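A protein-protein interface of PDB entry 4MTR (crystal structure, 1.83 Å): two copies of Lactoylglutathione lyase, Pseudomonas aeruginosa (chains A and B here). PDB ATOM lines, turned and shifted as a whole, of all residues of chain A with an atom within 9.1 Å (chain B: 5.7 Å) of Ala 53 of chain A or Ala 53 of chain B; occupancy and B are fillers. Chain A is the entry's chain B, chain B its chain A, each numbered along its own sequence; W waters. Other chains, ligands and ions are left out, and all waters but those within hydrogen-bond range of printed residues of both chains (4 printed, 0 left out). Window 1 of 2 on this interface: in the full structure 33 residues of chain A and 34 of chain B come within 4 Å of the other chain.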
ATOM      1  N   MET A   1      19.688 -16.856  16.968  1.00  0.00           N
ATOM      2  CA  MET A   1      18.958 -17.186  18.205  1.00  0.00           C
ATOM      3  C   MET A   1      18.666 -18.671  18.242  1.00  0.00           C
ATOM      4  O   MET A   1      18.656 -19.317  17.190  1.00  0.00           O
ATOM      5  CB  MET A   1      17.637 -16.418  18.263  1.00  0.00           C
ATOM      6  CG  MET A   1      17.834 -14.932  18.342  1.00  0.00           C
ATOM      7  SD  MET A   1      16.354 -13.997  17.965  1.00  0.00           S
ATOM      8  CE  MET A   1      15.394 -14.250  19.401  1.00  0.00           C
ATOM      9  N   ARG A   2      18.429 -19.217  19.445  1.00  0.00           N
ATOM     10  CA  ARG A   2      18.119 -20.639  19.582  1.00  0.00           C
ATOM     11  C   ARG A   2      17.301 -20.929  20.852  1.00  0.00           C
ATOM     12  O   ARG A   2      17.372 -20.178  21.830  1.00  0.00           O
ATOM     13  CB  ARG A   2      19.409 -21.495  19.541  1.00  0.00           C
ATOM     14  CG  ARG A   2      20.392 -21.151  20.638  1.00  0.00           C
ATOM     15  CD  ARG A   2      21.580 -22.064  20.639  1.00  0.00           C
ATOM     16  NE  ARG A   2      22.445 -21.782  21.786  1.00  0.00           N
ATOM     17  CZ  ARG A   2      22.776 -22.670  22.717  1.00  0.00           C
ATOM     18  NH1 ARG A   2      22.263 -23.891  22.692  1.00  0.00           N
ATOM     19  NH2 ARG A   2      23.566 -22.320  23.720  1.00  0.00           N
ATOM     20  N   ILE A   3      16.516 -22.001  20.825  1.00  0.00           N
ATOM     21  CA  ILE A   3      15.765 -22.442  22.002  1.00  0.00           C
ATOM     22  C   ILE A   3      16.763 -23.150  22.919  1.00  0.00           C
ATOM     23  O   ILE A   3      17.454 -24.067  22.480  1.00  0.00           O
ATOM     24  CB  ILE A   3      14.538 -23.347  21.611  1.00  0.00           C
ATOM     25  CG1 ILE A   3      13.486 -22.520  20.835  1.00  0.00           C
ATOM     26  CG2 ILE A   3      13.940 -24.031  22.862  1.00  0.00           C
ATOM     27  CD1 ILE A   3      12.386 -23.284  20.029  1.00  0.00           C
ATOM     28  N   LEU A   4      16.818 -22.732  24.185  1.00  0.00           N
ATOM     29  CA  LEU A   4      17.720 -23.300  25.173  1.00  0.00           C
ATOM     30  C   LEU A   4      17.048 -24.427  25.953  1.00  0.00           C
ATOM     31  O   LEU A   4      17.623 -25.496  26.085  1.00  0.00           O
ATOM     32  CB  LEU A   4      18.241 -22.212  26.133  1.00  0.00           C
ATOM     33  CG  LEU A   4      19.129 -21.117  25.492  1.00  0.00           C
ATOM     34  CD1 LEU A   4      19.311 -19.941  26.434  1.00  0.00           C
ATOM     35  CD2 LEU A   4      20.467 -21.676  25.055  1.00  0.00           C
ATOM     36  N   HIS A   5      15.831 -24.200  26.473  1.00  0.00           N
ATOM     37  CA  HIS A   5      15.167 -25.229  27.272  1.00  0.00           C
ATOM     38  C   HIS A   5      13.742 -24.883  27.577  1.00  0.00           C
ATOM     39  O   HIS A   5      13.386 -23.700  27.517  1.00  0.00           O
ATOM     40  CB  HIS A   5      15.910 -25.400  28.630  1.00  0.00           C
ATOM     41  CG  HIS A   5      16.029 -24.157  29.473  1.00  0.00           C
ATOM     42  ND1 HIS A   5      17.190 -23.407  29.492  1.00  0.00           N
ATOM     43  CD2 HIS A   5      15.162 -23.627  30.375  1.00  0.00           C
ATOM     44  CE1 HIS A   5      17.005 -22.473  30.414  1.00  0.00           C
ATOM     45  NE2 HIS A   5      15.801 -22.551  30.958  1.00  0.00           N
ATOM     46  N   SER A   6      12.923 -25.898  27.947  1.00  0.00           N
ATOM     47  CA  SER A   6      11.603 -25.643  28.541  1.00  0.00           C
ATOM     48  C   SER A   6      11.838 -25.861  30.018  1.00  0.00           C
ATOM     49  O   SER A   6      12.717 -26.649  30.384  1.00  0.00           O
ATOM     50  CB  SER A   6      10.564 -26.669  28.085  1.00  0.00           C
ATOM     51  OG  SER A   6      10.353 -26.670  26.684  1.00  0.00           O
ATOM     52  N   MET A  26      18.435 -39.591  29.312  1.00  0.00           N
ATOM     53  CA  MET A  26      18.962 -38.240  29.408  1.00  0.00           C
ATOM     54  C   MET A  26      20.089 -38.241  30.418  1.00  0.00           C
ATOM     55  O   MET A  26      20.121 -39.096  31.305  1.00  0.00           O
ATOM     56  CB  MET A  26      17.880 -37.249  29.861  1.00  0.00           C
ATOM     57  CG  MET A  26      16.863 -36.917  28.805  1.00  0.00           C
ATOM     58  SD  MET A  26      15.844 -35.516  29.309  1.00  0.00           S
ATOM     59  CE  MET A  26      14.769 -35.411  27.882  1.00  0.00           C
ATOM     60  N   LEU A  29      22.700 -32.834  33.407  1.00  0.00           N
ATOM     61  CA  LEU A  29      23.689 -31.840  32.948  1.00  0.00           C
ATOM     62  C   LEU A  29      24.210 -30.949  34.051  1.00  0.00           C
ATOM     63  O   LEU A  29      25.357 -30.518  33.994  1.00  0.00           O
ATOM     64  CB  LEU A  29      23.130 -30.990  31.800  1.00  0.00           C
ATOM     65  CG  LEU A  29      22.582 -31.725  30.579  1.00  0.00           C
ATOM     66  CD1 LEU A  29      22.008 -30.760  29.610  1.00  0.00           C
ATOM     67  CD2 LEU A  29      23.640 -32.584  29.903  1.00  0.00           C
ATOM     68  N   PHE A  43      19.148 -29.685  35.313  1.00  0.00           N
ATOM     69  CA  PHE A  43      19.039 -29.623  33.873  1.00  0.00           C
ATOM     70  C   PHE A  43      19.369 -30.997  33.371  1.00  0.00           C
ATOM     71  O   PHE A  43      20.355 -31.586  33.828  1.00  0.00           O
ATOM     72  CB  PHE A  43      19.996 -28.596  33.276  1.00  0.00           C
ATOM     73  CG  PHE A  43      19.464 -27.194  33.323  1.00  0.00           C
ATOM     74  CD1 PHE A  43      19.684 -26.389  34.430  1.00  0.00           C
ATOM     75  CD2 PHE A  43      18.773 -26.660  32.239  1.00  0.00           C
ATOM     76  CE1 PHE A  43      19.196 -25.072  34.469  1.00  0.00           C
ATOM     77  CE2 PHE A  43      18.303 -25.343  32.274  1.00  0.00           C
ATOM     78  CZ  PHE A  43      18.531 -24.554  33.389  1.00  0.00           C
ATOM     79  N   VAL A  44      18.514 -31.520  32.469  1.00  0.00           N
ATOM     80  CA  VAL A  44      18.650 -32.833  31.848  1.00  0.00           C
ATOM     81  C   VAL A  44      18.597 -32.696  30.343  1.00  0.00           C
ATOM     82  O   VAL A  44      17.887 -31.842  29.818  1.00  0.00           O
ATOM     83  CB  VAL A  44      17.640 -33.885  32.380  1.00  0.00           C
ATOM     84  CG1 VAL A  44      17.910 -34.183  33.850  1.00  0.00           C
ATOM     85  CG2 VAL A  44      16.184 -33.438  32.194  1.00  0.00           C
ATOM     86  N   GLY A  45      19.296 -33.574  29.646  1.00  0.00           N
ATOM     87  CA  GLY A  45      19.327 -33.531  28.192  1.00  0.00           C
ATOM     88  C   GLY A  45      20.264 -34.552  27.598  1.00  0.00           C
ATOM     89  O   GLY A  45      20.714 -35.468  28.287  1.00  0.00           O
ATOM     90  N   TYR A  46      20.548 -34.402  26.321  1.00  0.00           N
ATOM     91  CA  TYR A  46      21.388 -35.329  25.567  1.00  0.00           C
ATOM     92  C   TYR A  46      22.724 -34.699  25.222  1.00  0.00           C
ATOM     93  O   TYR A  46      23.751 -35.318  25.462  1.00  0.00           O
ATOM     94  CB  TYR A  46      20.634 -35.817  24.329  1.00  0.00           C
ATOM     95  CG  TYR A  46      19.313 -36.471  24.690  1.00  0.00           C
ATOM     96  CD1 TYR A  46      19.275 -37.723  25.298  1.00  0.00           C
ATOM     97  CD2 TYR A  46      18.102 -35.817  24.462  1.00  0.00           C
ATOM     98  CE1 TYR A  46      18.066 -38.320  25.645  1.00  0.00           C
ATOM     99  CE2 TYR A  46      16.887 -36.411  24.789  1.00  0.00           C
ATOM    100  CZ  TYR A  46      16.875 -37.661  25.385  1.00  0.00           C
ATOM    101  OH  TYR A  46      15.685 -38.254  25.715  1.00  0.00           O
ATOM    102  N   GLN A  47      22.718 -33.456  24.722  1.00  0.00           N
ATOM    103  CA  GLN A  47      23.951 -32.715  24.429  1.00  0.00           C
ATOM    104  C   GLN A  47      24.142 -31.638  25.477  1.00  0.00           C
ATOM    105  O   GLN A  47      23.201 -31.341  26.224  1.00  0.00           O
ATOM    106  CB  GLN A  47      23.901 -32.107  23.027  1.00  0.00           C
ATOM    107  CG  GLN A  47      24.043 -33.136  21.908  1.00  0.00           C
ATOM    108  CD  GLN A  47      24.109 -32.485  20.545  1.00  0.00           C
ATOM    109  N   ASP A  48      25.357 -31.051  25.562  1.00  0.00           N
ATOM    110  CA  ASP A  48      25.591 -29.943  26.489  1.00  0.00           C
ATOM    111  C   ASP A  48      24.734 -28.761  26.031  1.00  0.00           C
ATOM    112  O   ASP A  48      24.413 -28.649  24.847  1.00  0.00           O
ATOM    113  CB  ASP A  48      27.080 -29.555  26.607  1.00  0.00           C
ATOM    114  CG  ASP A  48      27.794 -29.375  25.288  1.00  0.00           C
ATOM    115  OD1 ASP A  48      27.709 -28.269  24.713  1.00  0.00           O
ATOM    116  OD2 ASP A  48      28.459 -30.332  24.841  1.00  0.00           O
ATOM    117  N   GLU A  49      24.312 -27.933  26.972  1.00  0.00           N
ATOM    118  CA  GLU A  49      23.443 -26.771  26.745  1.00  0.00           C
ATOM    119  C   GLU A  49      23.913 -25.797  25.652  1.00  0.00           C
ATOM    120  O   GLU A  49      23.077 -25.085  25.062  1.00  0.00           O
ATOM    121  CB  GLU A  49      23.177 -26.037  28.062  1.00  0.00           C
ATOM    122  CG  GLU A  49      22.707 -26.952  29.182  1.00  0.00           C
ATOM    123  CD  GLU A  49      23.765 -27.243  30.228  1.00  0.00           C
ATOM    124  OE1 GLU A  49      24.720 -28.003  29.944  1.00  0.00           O
ATOM    125  OE2 GLU A  49      23.626 -26.705  31.348  1.00  0.00           O
ATOM    126  N   ARG A  50      25.246 -25.767  25.384  1.00  0.00           N
ATOM    127  CA  ARG A  50      25.841 -24.910  24.348  1.00  0.00           C
ATOM    128  C   ARG A  50      25.493 -25.409  22.957  1.00  0.00           C
ATOM    129  O   ARG A  50      25.493 -24.612  22.026  1.00  0.00           O
ATOM    130  CB  ARG A  50      27.379 -24.859  24.480  1.00  0.00           C
ATOM    131  CG  ARG A  50      27.910 -23.964  25.580  1.00  0.00           C
ATOM    132  CD  ARG A  50      29.428 -24.065  25.682  1.00  0.00           C
ATOM    133  NE  ARG A  50      30.014 -22.860  26.274  1.00  0.00           N
ATOM    134  CZ  ARG A  50      31.285 -22.738  26.650  1.00  0.00           C
ATOM    135  NH1 ARG A  50      32.129 -23.755  26.511  1.00  0.00           N
ATOM    136  NH2 ARG A  50      31.720 -21.601  27.179  1.00  0.00           N
ATOM    137  N   ALA A  51      25.212 -26.721  22.804  1.00  0.00           N
ATOM    138  CA  ALA A  51      24.927 -27.330  21.505  1.00  0.00           C
ATOM    139  C   ALA A  51      23.455 -27.554  21.158  1.00  0.00           C
ATOM    140  O   ALA A  51      23.080 -27.461  19.982  1.00  0.00           O
ATOM    141  CB  ALA A  51      25.674 -28.647  21.383  1.00  0.00           C
ATOM    142  N   ALA A  52      22.635 -27.922  22.158  1.00  0.00           N
ATOM    143  CA  ALA A  52      21.254 -28.290  21.903  1.00  0.00           C
ATOM    144  C   ALA A  52      20.352 -27.856  23.038  1.00  0.00           C
ATOM    145  O   ALA A  52      20.850 -27.464  24.081  1.00  0.00           O
ATOM    146  CB  ALA A  52      21.179 -29.809  21.735  1.00  0.00           C
ATOM    147  N   ALA A  53      19.017 -27.974  22.848  1.00  0.00           N
ATOM    148  CA  ALA A  53      18.012 -27.669  23.866  1.00  0.00           C
ATOM    149  C   ALA A  53      18.056 -28.725  24.947  1.00  0.00           C
ATOM    150  O   ALA A  53      18.261 -29.894  24.635  1.00  0.00           O
ATOM    151  CB  ALA A  53      16.614 -27.647  23.240  1.00  0.00           C
ATOM    152  N   ALA A  54      17.841 -28.321  26.200  1.00  0.00           N
ATOM    153  CA  ALA A  54      17.793 -29.203  27.383  1.00  0.00           C
ATOM    154  C   ALA A  54      16.401 -29.092  28.035  1.00  0.00           C
ATOM    155  O   ALA A  54      15.529 -28.379  27.534  1.00  0.00           O
ATOM    156  CB  ALA A  54      18.862 -28.767  28.377  1.00  0.00           C
ATOM    157  N   LEU A  55      16.200 -29.782  29.152  1.00  0.00           N
ATOM    158  CA  LEU A  55      14.979 -29.697  29.925  1.00  0.00           C
ATOM    159  C   LEU A  55      15.339 -29.284  31.336  1.00  0.00           C
ATOM    160  O   LEU A  55      16.175 -29.935  31.960  1.00  0.00           O
ATOM    161  CB  LEU A  55      14.190 -31.026  29.912  1.00  0.00           C
ATOM    162  CG  LEU A  55      13.024 -31.135  30.894  1.00  0.00           C
ATOM    163  CD1 LEU A  55      11.853 -30.216  30.480  1.00  0.00           C
ATOM    164  CD2 LEU A  55      12.519 -32.572  30.958  1.00  0.00           C
ATOM    165  N   GLU A  56      14.735 -28.193  31.827  1.00  0.00           N
ATOM    166  CA  GLU A  56      14.947 -27.716  33.181  1.00  0.00           C
ATOM    167  C   GLU A  56      13.825 -28.223  34.080  1.00  0.00           C
ATOM    168  O   GLU A  56      12.637 -28.064  33.759  1.00  0.00           O
ATOM    169  CB  GLU A  56      14.965 -26.182  33.214  1.00  0.00           C
ATOM    170  CG  GLU A  56      15.322 -25.588  34.587  1.00  0.00           C
ATOM    171  CD  GLU A  56      15.297 -24.068  34.554  1.00  0.00           C
ATOM    172  OE1 GLU A  56      14.964 -23.517  33.482  1.00  0.00           O
ATOM    173  OE2 GLU A  56      15.642 -23.427  35.572  1.00  0.00           O
ATOM    174  N   LEU A  75       6.345 -32.611  25.510  1.00  0.00           N
ATOM    175  CA  LEU A  75       7.731 -32.511  25.086  1.00  0.00           C
ATOM    176  C   LEU A  75       7.939 -33.678  24.119  1.00  0.00           C
ATOM    177  O   LEU A  75       7.622 -34.821  24.461  1.00  0.00           O
ATOM    178  CB  LEU A  75       8.692 -32.663  26.273  1.00  0.00           C
ATOM    179  CG  LEU A  75      10.189 -32.447  25.917  1.00  0.00           C
ATOM    180  CD1 LEU A  75      10.452 -30.992  25.522  1.00  0.00           C
ATOM    181  CD2 LEU A  75      11.094 -32.852  27.097  1.00  0.00           C
ATOM    182  N   ALA A  76       8.416 -33.385  22.915  1.00  0.00           N
ATOM    183  CA  ALA A  76       8.690 -34.408  21.905  1.00  0.00           C
ATOM    184  C   ALA A  76      10.163 -34.680  21.882  1.00  0.00           C
ATOM    185  O   ALA A  76      10.990 -33.752  22.017  1.00  0.00           O
ATOM    186  CB  ALA A  76       8.224 -33.950  20.530  1.00  0.00           C
ATOM    187  N   ILE A  77      10.497 -35.973  21.807  1.00  0.00           N
ATOM    188  CA  ILE A  77      11.857 -36.481  21.787  1.00  0.00           C
ATOM    189  C   ILE A  77      12.030 -37.398  20.619  1.00  0.00           C
ATOM    190  O   ILE A  77      11.172 -38.263  20.370  1.00  0.00           O
ATOM    191  CB  ILE A  77      12.255 -37.159  23.133  1.00  0.00           C
ATOM    192  CG1 ILE A  77      12.288 -36.109  24.264  1.00  0.00           C
ATOM    193  CG2 ILE A  77      13.656 -37.845  23.017  1.00  0.00           C
ATOM    194  CD1 ILE A  77      12.247 -36.638  25.546  1.00  0.00           C
ATOM    195  N   ARG B   2      17.332 -36.755  20.717  1.00  0.00           N
ATOM    196  CA  ARG B   2      17.365 -35.300  20.854  1.00  0.00           C
ATOM    197  C   ARG B   2      15.994 -34.738  21.163  1.00  0.00           C
ATOM    198  O   ARG B   2      14.975 -35.334  20.789  1.00  0.00           O
ATOM    199  CB  ARG B   2      17.969 -34.611  19.616  1.00  0.00           C
ATOM    200  CG  ARG B   2      17.165 -34.774  18.377  1.00  0.00           C
ATOM    201  CD  ARG B   2      17.872 -34.167  17.197  1.00  0.00           C
ATOM    202  NE  ARG B   2      17.060 -34.426  16.020  1.00  0.00           N
ATOM    203  CZ  ARG B   2      16.327 -33.519  15.403  1.00  0.00           C
ATOM    204  NH1 ARG B   2      16.350 -32.253  15.800  1.00  0.00           N
ATOM    205  NH2 ARG B   2      15.577 -33.863  14.370  1.00  0.00           N
ATOM    206  N   ILE B   3      15.964 -33.574  21.823  1.00  0.00           N
ATOM    207  CA  ILE B   3      14.671 -32.927  22.076  1.00  0.00           C
ATOM    208  C   ILE B   3      14.253 -32.267  20.763  1.00  0.00           C
ATOM    209  O   ILE B   3      15.051 -31.538  20.164  1.00  0.00           O
ATOM    210  CB  ILE B   3      14.730 -31.935  23.278  1.00  0.00           C
ATOM    211  CG1 ILE B   3      14.918 -32.672  24.613  1.00  0.00           C
ATOM    212  CG2 ILE B   3      13.473 -31.079  23.319  1.00  0.00           C
ATOM    213  CD1 ILE B   3      15.520 -31.772  25.759  1.00  0.00           C
ATOM    214  N   LEU B   4      13.006 -32.531  20.315  1.00  0.00           N
ATOM    215  CA  LEU B   4      12.470 -32.004  19.063  1.00  0.00           C
ATOM    216  C   LEU B   4      11.714 -30.734  19.257  1.00  0.00           C
ATOM    217  O   LEU B   4      11.914 -29.793  18.487  1.00  0.00           O
ATOM    218  CB  LEU B   4      11.527 -33.025  18.402  1.00  0.00           C
ATOM    219  CG  LEU B   4      12.187 -34.299  17.913  1.00  0.00           C
ATOM    220  CD1 LEU B   4      11.138 -35.275  17.422  1.00  0.00           C
ATOM    221  CD2 LEU B   4      13.235 -34.007  16.830  1.00  0.00           C
ATOM    222  N   HIS B   5      10.787 -30.716  20.247  1.00  0.00           N
ATOM    223  CA  HIS B   5       9.949 -29.537  20.488  1.00  0.00           C
ATOM    224  C   HIS B   5       9.137 -29.668  21.777  1.00  0.00           C
ATOM    225  O   HIS B   5       8.972 -30.765  22.288  1.00  0.00           O
ATOM    226  CB  HIS B   5       8.982 -29.277  19.270  1.00  0.00           C
ATOM    227  CG  HIS B   5       7.998 -30.381  18.987  1.00  0.00           C
ATOM    228  ND1 HIS B   5       8.241 -31.346  18.001  1.00  0.00           N
ATOM    229  CD2 HIS B   5       6.814 -30.669  19.590  1.00  0.00           C
ATOM    230  CE1 HIS B   5       7.173 -32.150  18.004  1.00  0.00           C
ATOM    231  NE2 HIS B   5       6.286 -31.789  18.939  1.00  0.00           N
ATOM    232  N   VAL B  44       7.111 -23.462  14.903  1.00  0.00           N
ATOM    233  CA  VAL B  44       7.917 -22.265  14.723  1.00  0.00           C
ATOM    234  C   VAL B  44       9.278 -22.495  15.302  1.00  0.00           C
ATOM    235  O   VAL B  44       9.429 -23.238  16.276  1.00  0.00           O
ATOM    236  CB  VAL B  44       7.254 -20.968  15.299  1.00  0.00           C
ATOM    237  CG1 VAL B  44       6.026 -20.575  14.491  1.00  0.00           C
ATOM    238  CG2 VAL B  44       6.914 -21.100  16.796  1.00  0.00           C
ATOM    239  N   GLY B  45      10.263 -21.821  14.743  1.00  0.00           N
ATOM    240  CA  GLY B  45      11.606 -21.890  15.284  1.00  0.00           C
ATOM    241  C   GLY B  45      12.616 -21.071  14.526  1.00  0.00           C
ATOM    242  O   GLY B  45      12.259 -20.162  13.773  1.00  0.00           O
ATOM    243  N   TYR B  46      13.871 -21.417  14.726  1.00  0.00           N
ATOM    244  CA  TYR B  46      15.036 -20.747  14.149  1.00  0.00           C
ATOM    245  C   TYR B  46      15.704 -21.544  13.047  1.00  0.00           C
ATOM    246  O   TYR B  46      15.890 -21.014  11.952  1.00  0.00           O
ATOM    247  CB  TYR B  46      15.997 -20.354  15.281  1.00  0.00           C
ATOM    248  CG  TYR B  46      15.324 -19.435  16.279  1.00  0.00           C
ATOM    249  CD1 TYR B  46      14.979 -18.133  15.936  1.00  0.00           C
ATOM    250  CD2 TYR B  46      14.986 -19.885  17.550  1.00  0.00           C
ATOM    251  CE1 TYR B  46      14.343 -17.294  16.843  1.00  0.00           C
ATOM    252  CE2 TYR B  46      14.362 -19.048  18.472  1.00  0.00           C
ATOM    253  CZ  TYR B  46      14.043 -17.754  18.115  1.00  0.00           C
ATOM    254  OH  TYR B  46      13.405 -16.933  19.020  1.00  0.00           O
ATOM    255  N   GLU B  49      13.651 -28.286  11.599  1.00  0.00           N
ATOM    256  CA  GLU B  49      13.396 -29.269  12.667  1.00  0.00           C
ATOM    257  C   GLU B  49      14.418 -30.400  12.732  1.00  0.00           C
ATOM    258  O   GLU B  49      14.673 -30.951  13.812  1.00  0.00           O
ATOM    259  CB  GLU B  49      11.983 -29.816  12.556  1.00  0.00           C
ATOM    260  CG  GLU B  49      10.929 -28.777  12.880  1.00  0.00           C
ATOM    261  CD  GLU B  49       9.540 -29.310  12.660  1.00  0.00           C
ATOM    262  OE1 GLU B  49       9.005 -29.986  13.570  1.00  0.00           O
ATOM    263  OE2 GLU B  49       8.994 -29.072  11.563  1.00  0.00           O
ATOM    264  N   ALA B  51      17.575 -29.991  12.473  1.00  0.00           N
ATOM    265  CA  ALA B  51      18.782 -29.422  13.104  1.00  0.00           C
ATOM    266  C   ALA B  51      18.637 -28.977  14.543  1.00  0.00           C
ATOM    267  O   ALA B  51      19.623 -28.963  15.289  1.00  0.00           O
ATOM    268  CB  ALA B  51      19.299 -28.247  12.265  1.00  0.00           C
ATOM    269  N   ALA B  52      17.452 -28.506  14.924  1.00  0.00           N
ATOM    270  CA  ALA B  52      17.290 -27.974  16.280  1.00  0.00           C
ATOM    271  C   ALA B  52      15.873 -28.114  16.794  1.00  0.00           C
ATOM    272  O   ALA B  52      14.952 -28.414  16.025  1.00  0.00           O
ATOM    273  CB  ALA B  52      17.697 -26.499  16.308  1.00  0.00           C
ATOM    274  N   ALA B  53      15.696 -27.827  18.095  1.00  0.00           N
ATOM    275  CA  ALA B  53      14.406 -27.878  18.787  1.00  0.00           C
ATOM    276  C   ALA B  53      13.524 -26.758  18.272  1.00  0.00           C
ATOM    277  O   ALA B  53      14.017 -25.651  18.080  1.00  0.00           O
ATOM    278  CB  ALA B  53      14.629 -27.688  20.272  1.00  0.00           C
ATOM    279  N   ALA B  54      12.223 -27.022  18.144  1.00  0.00           N
ATOM    280  CA  ALA B  54      11.215 -26.069  17.700  1.00  0.00           C
ATOM    281  C   ALA B  54      10.157 -25.910  18.769  1.00  0.00           C
ATOM    282  O   ALA B  54      10.265 -26.461  19.881  1.00  0.00           O
ATOM    283  CB  ALA B  54      10.572 -26.556  16.400  1.00  0.00           C
ATOM    284  N   LEU B  55       9.180 -25.084  18.474  1.00  0.00           N
ATOM    285  CA  LEU B  55       8.048 -24.838  19.354  1.00  0.00           C
ATOM    286  C   LEU B  55       6.796 -25.168  18.560  1.00  0.00           C
ATOM    287  O   LEU B  55       6.602 -24.627  17.469  1.00  0.00           O
ATOM    288  CB  LEU B  55       8.028 -23.373  19.846  1.00  0.00           C
ATOM    289  CG  LEU B  55       6.785 -22.968  20.664  1.00  0.00           C
ATOM    290  CD1 LEU B  55       6.680 -23.793  21.995  1.00  0.00           C
ATOM    291  CD2 LEU B  55       6.758 -21.453  20.913  1.00  0.00           C
HETATM  292  O   HOH W   1      16.509 -23.683  18.292  1.00  0.00           O
HETATM  293  O   HOH W   2      18.529 -32.337  22.480  1.00  0.00           O
HETATM  294  O   HOH W   3      20.518 -28.133  18.078  1.00  0.00           O
HETATM  295  O   HOH W   4      18.260 -27.958  19.729  1.00  0.00           O
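The backbone carbonyl oxygen of Ala 76 of chain A sits at hydrogen-bond distance from the backbone NH of Leu 4 of chain B, at 2.9 Å. The backbone NH (N) of Ala 76 of chain A sits at hydrogen-bond distance from the backbone carbonyl oxygen (O) of His 5 of chain B, at 2.8 Å.
The backbone carbonyl oxygen (O) of Leu 4 of chain B lies within hydrogen-bond range of the backbone NH (N) of Ala 54 of chain B. The backbone carbonyl oxygen of Val 44 of chain A sits at hydrogen-bond distance from the backbone NH of Leu 55 of chain A (2.7 Å). N of Val 44 of chain B sits at hydrogen-bond distance from O of Leu 55 of chain B (2.9 Å). The backbone carbonyl oxygen of Glu 49 of chain A lies within hydrogen-bond range of the guanidinium group of Arg 2 of chain A (2.8 Å). The guanidinium group (NH1) of Arg 2 of chain A sits at hydrogen-bond distance from the backbone carbonyl oxygen (O) of Arg 50 of chain A (3.4 Å). O of Leu 4 of chain A lies within hydrogen-bond range of N of Ala 54 of chain A, 2.8 Å away.
Arg 2 of chain A touches Tyr 46 of chain B (CA to CD2, 3.8 Å). CD1 of Ile 3 of chain A touches O of Ala 53 of chain B, 3.5 Å away. CD1 of Ile 3 of chain A touches N of Leu 55 of chain B, at 3.99 Å. Tyr 46 of chain A touches Arg 2 of chain B. CD1 of Ile 3 of chain B touches O of Ala 53 of chain A (3.5 Å). Ala 53 of chain A touches Ala 53 of chain B. C of Ala 54 of chain A touches CD1 of Ile 3 of chain B (3.6 Å). Ile 3 of chain B touches Leu 75 of chain A (CG2 to CD1, 3.7 Å). Ala 76 of chain A touches Ile 3 of chain B. Arg 2 of chain B touches Ile 77 of chain A (O to CA, 3.5 Å).
Of the printed residues of chain B, Ile 3 of chain A touches Ala 53, Ala 54 and Leu 55. Of the printed residues of chain B, Tyr 46 of chain A touches Arg 2. Ala 52 of chain A touches none of the printed residues of chain B. Of the printed residues of chain B, Ala 53 of chain A touches Ile 3 (3.5 Å) and Ala 53 (3.6 Å). Printed residues of chain B within 4 Å of Leu 75 of chain A: Ile 3 (3.7 Å) and His 5 (3.5 Å). Printed residues of chain A within 4 Å of Tyr 46 of chain B: Met 1 (3.4 Å) and Arg 2 (3.8 Å). No residue of chain A comes within 4 Å of Ala 52 of chain B. Ala 53 of chain B touches just these residues of chain A: Ile 3 (3.5 Å) and Ala 53 (3.6 Å). Ala 54 of chain B touches just one residue of chain A: Ile 3 (3.7 Å). The nearest printed residue of chain A that does not touch Ala 53 of chain B is Ala 52 of chain A (6.4 Å).
Hydrophobic or aromatic side chains of chain B within 4 Å of the printed part of chain A: Ile 3, Leu 4, His 5, Tyr 46 and Ala 53. Hydrophobic or aromatic side chains of chain A within 4 Å of the printed part of chain B: Met 1, Ile 3, Tyr 46, Ala 53, Leu 75, Ala 76 and Ile 77.
Arg 2 of chain A touches Tyr 46 of chain B, and with the chains exchanged Tyr 46 of chain A touches Arg 2 of chain B. Ile 3 of chain A touches Ala 54 of chain B, and with the chains exchanged Ala 54 of chain A touches Ile 3 of chain B. Ile 3 of chain A touches Leu 55 of chain B, and with the chains exchanged Leu 55 of chain A touches Ile 3 of chain B. Ala 53 of chain B touches its own counterpart, Ala 53 of chain A. Positions printed for both chains: 2, 3, 4, 5, 44, 45, 46, 49, 51, 52, 53, 54 and 55.
Water W2 lies within hydrogen-bond range of N of Ile 3 of chain B and O of Ala 53 of chain A. Water W1 lies within hydrogen-bond range of the backbone NH (N) of Ile 3 of chain A (3.0 Å) and the backbone carbonyl oxygen (O) of Ala 53 of chain B (3.2 Å). Water W4 bridges the backbone NH of Ala 53 of chain B and the backbone NH of Ala 53 of chain A. Water W3 bridges the backbone carbonyl oxygen of Ala 51 of chain B and the backbone carbonyl oxygen of Ala 51 of chain A.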
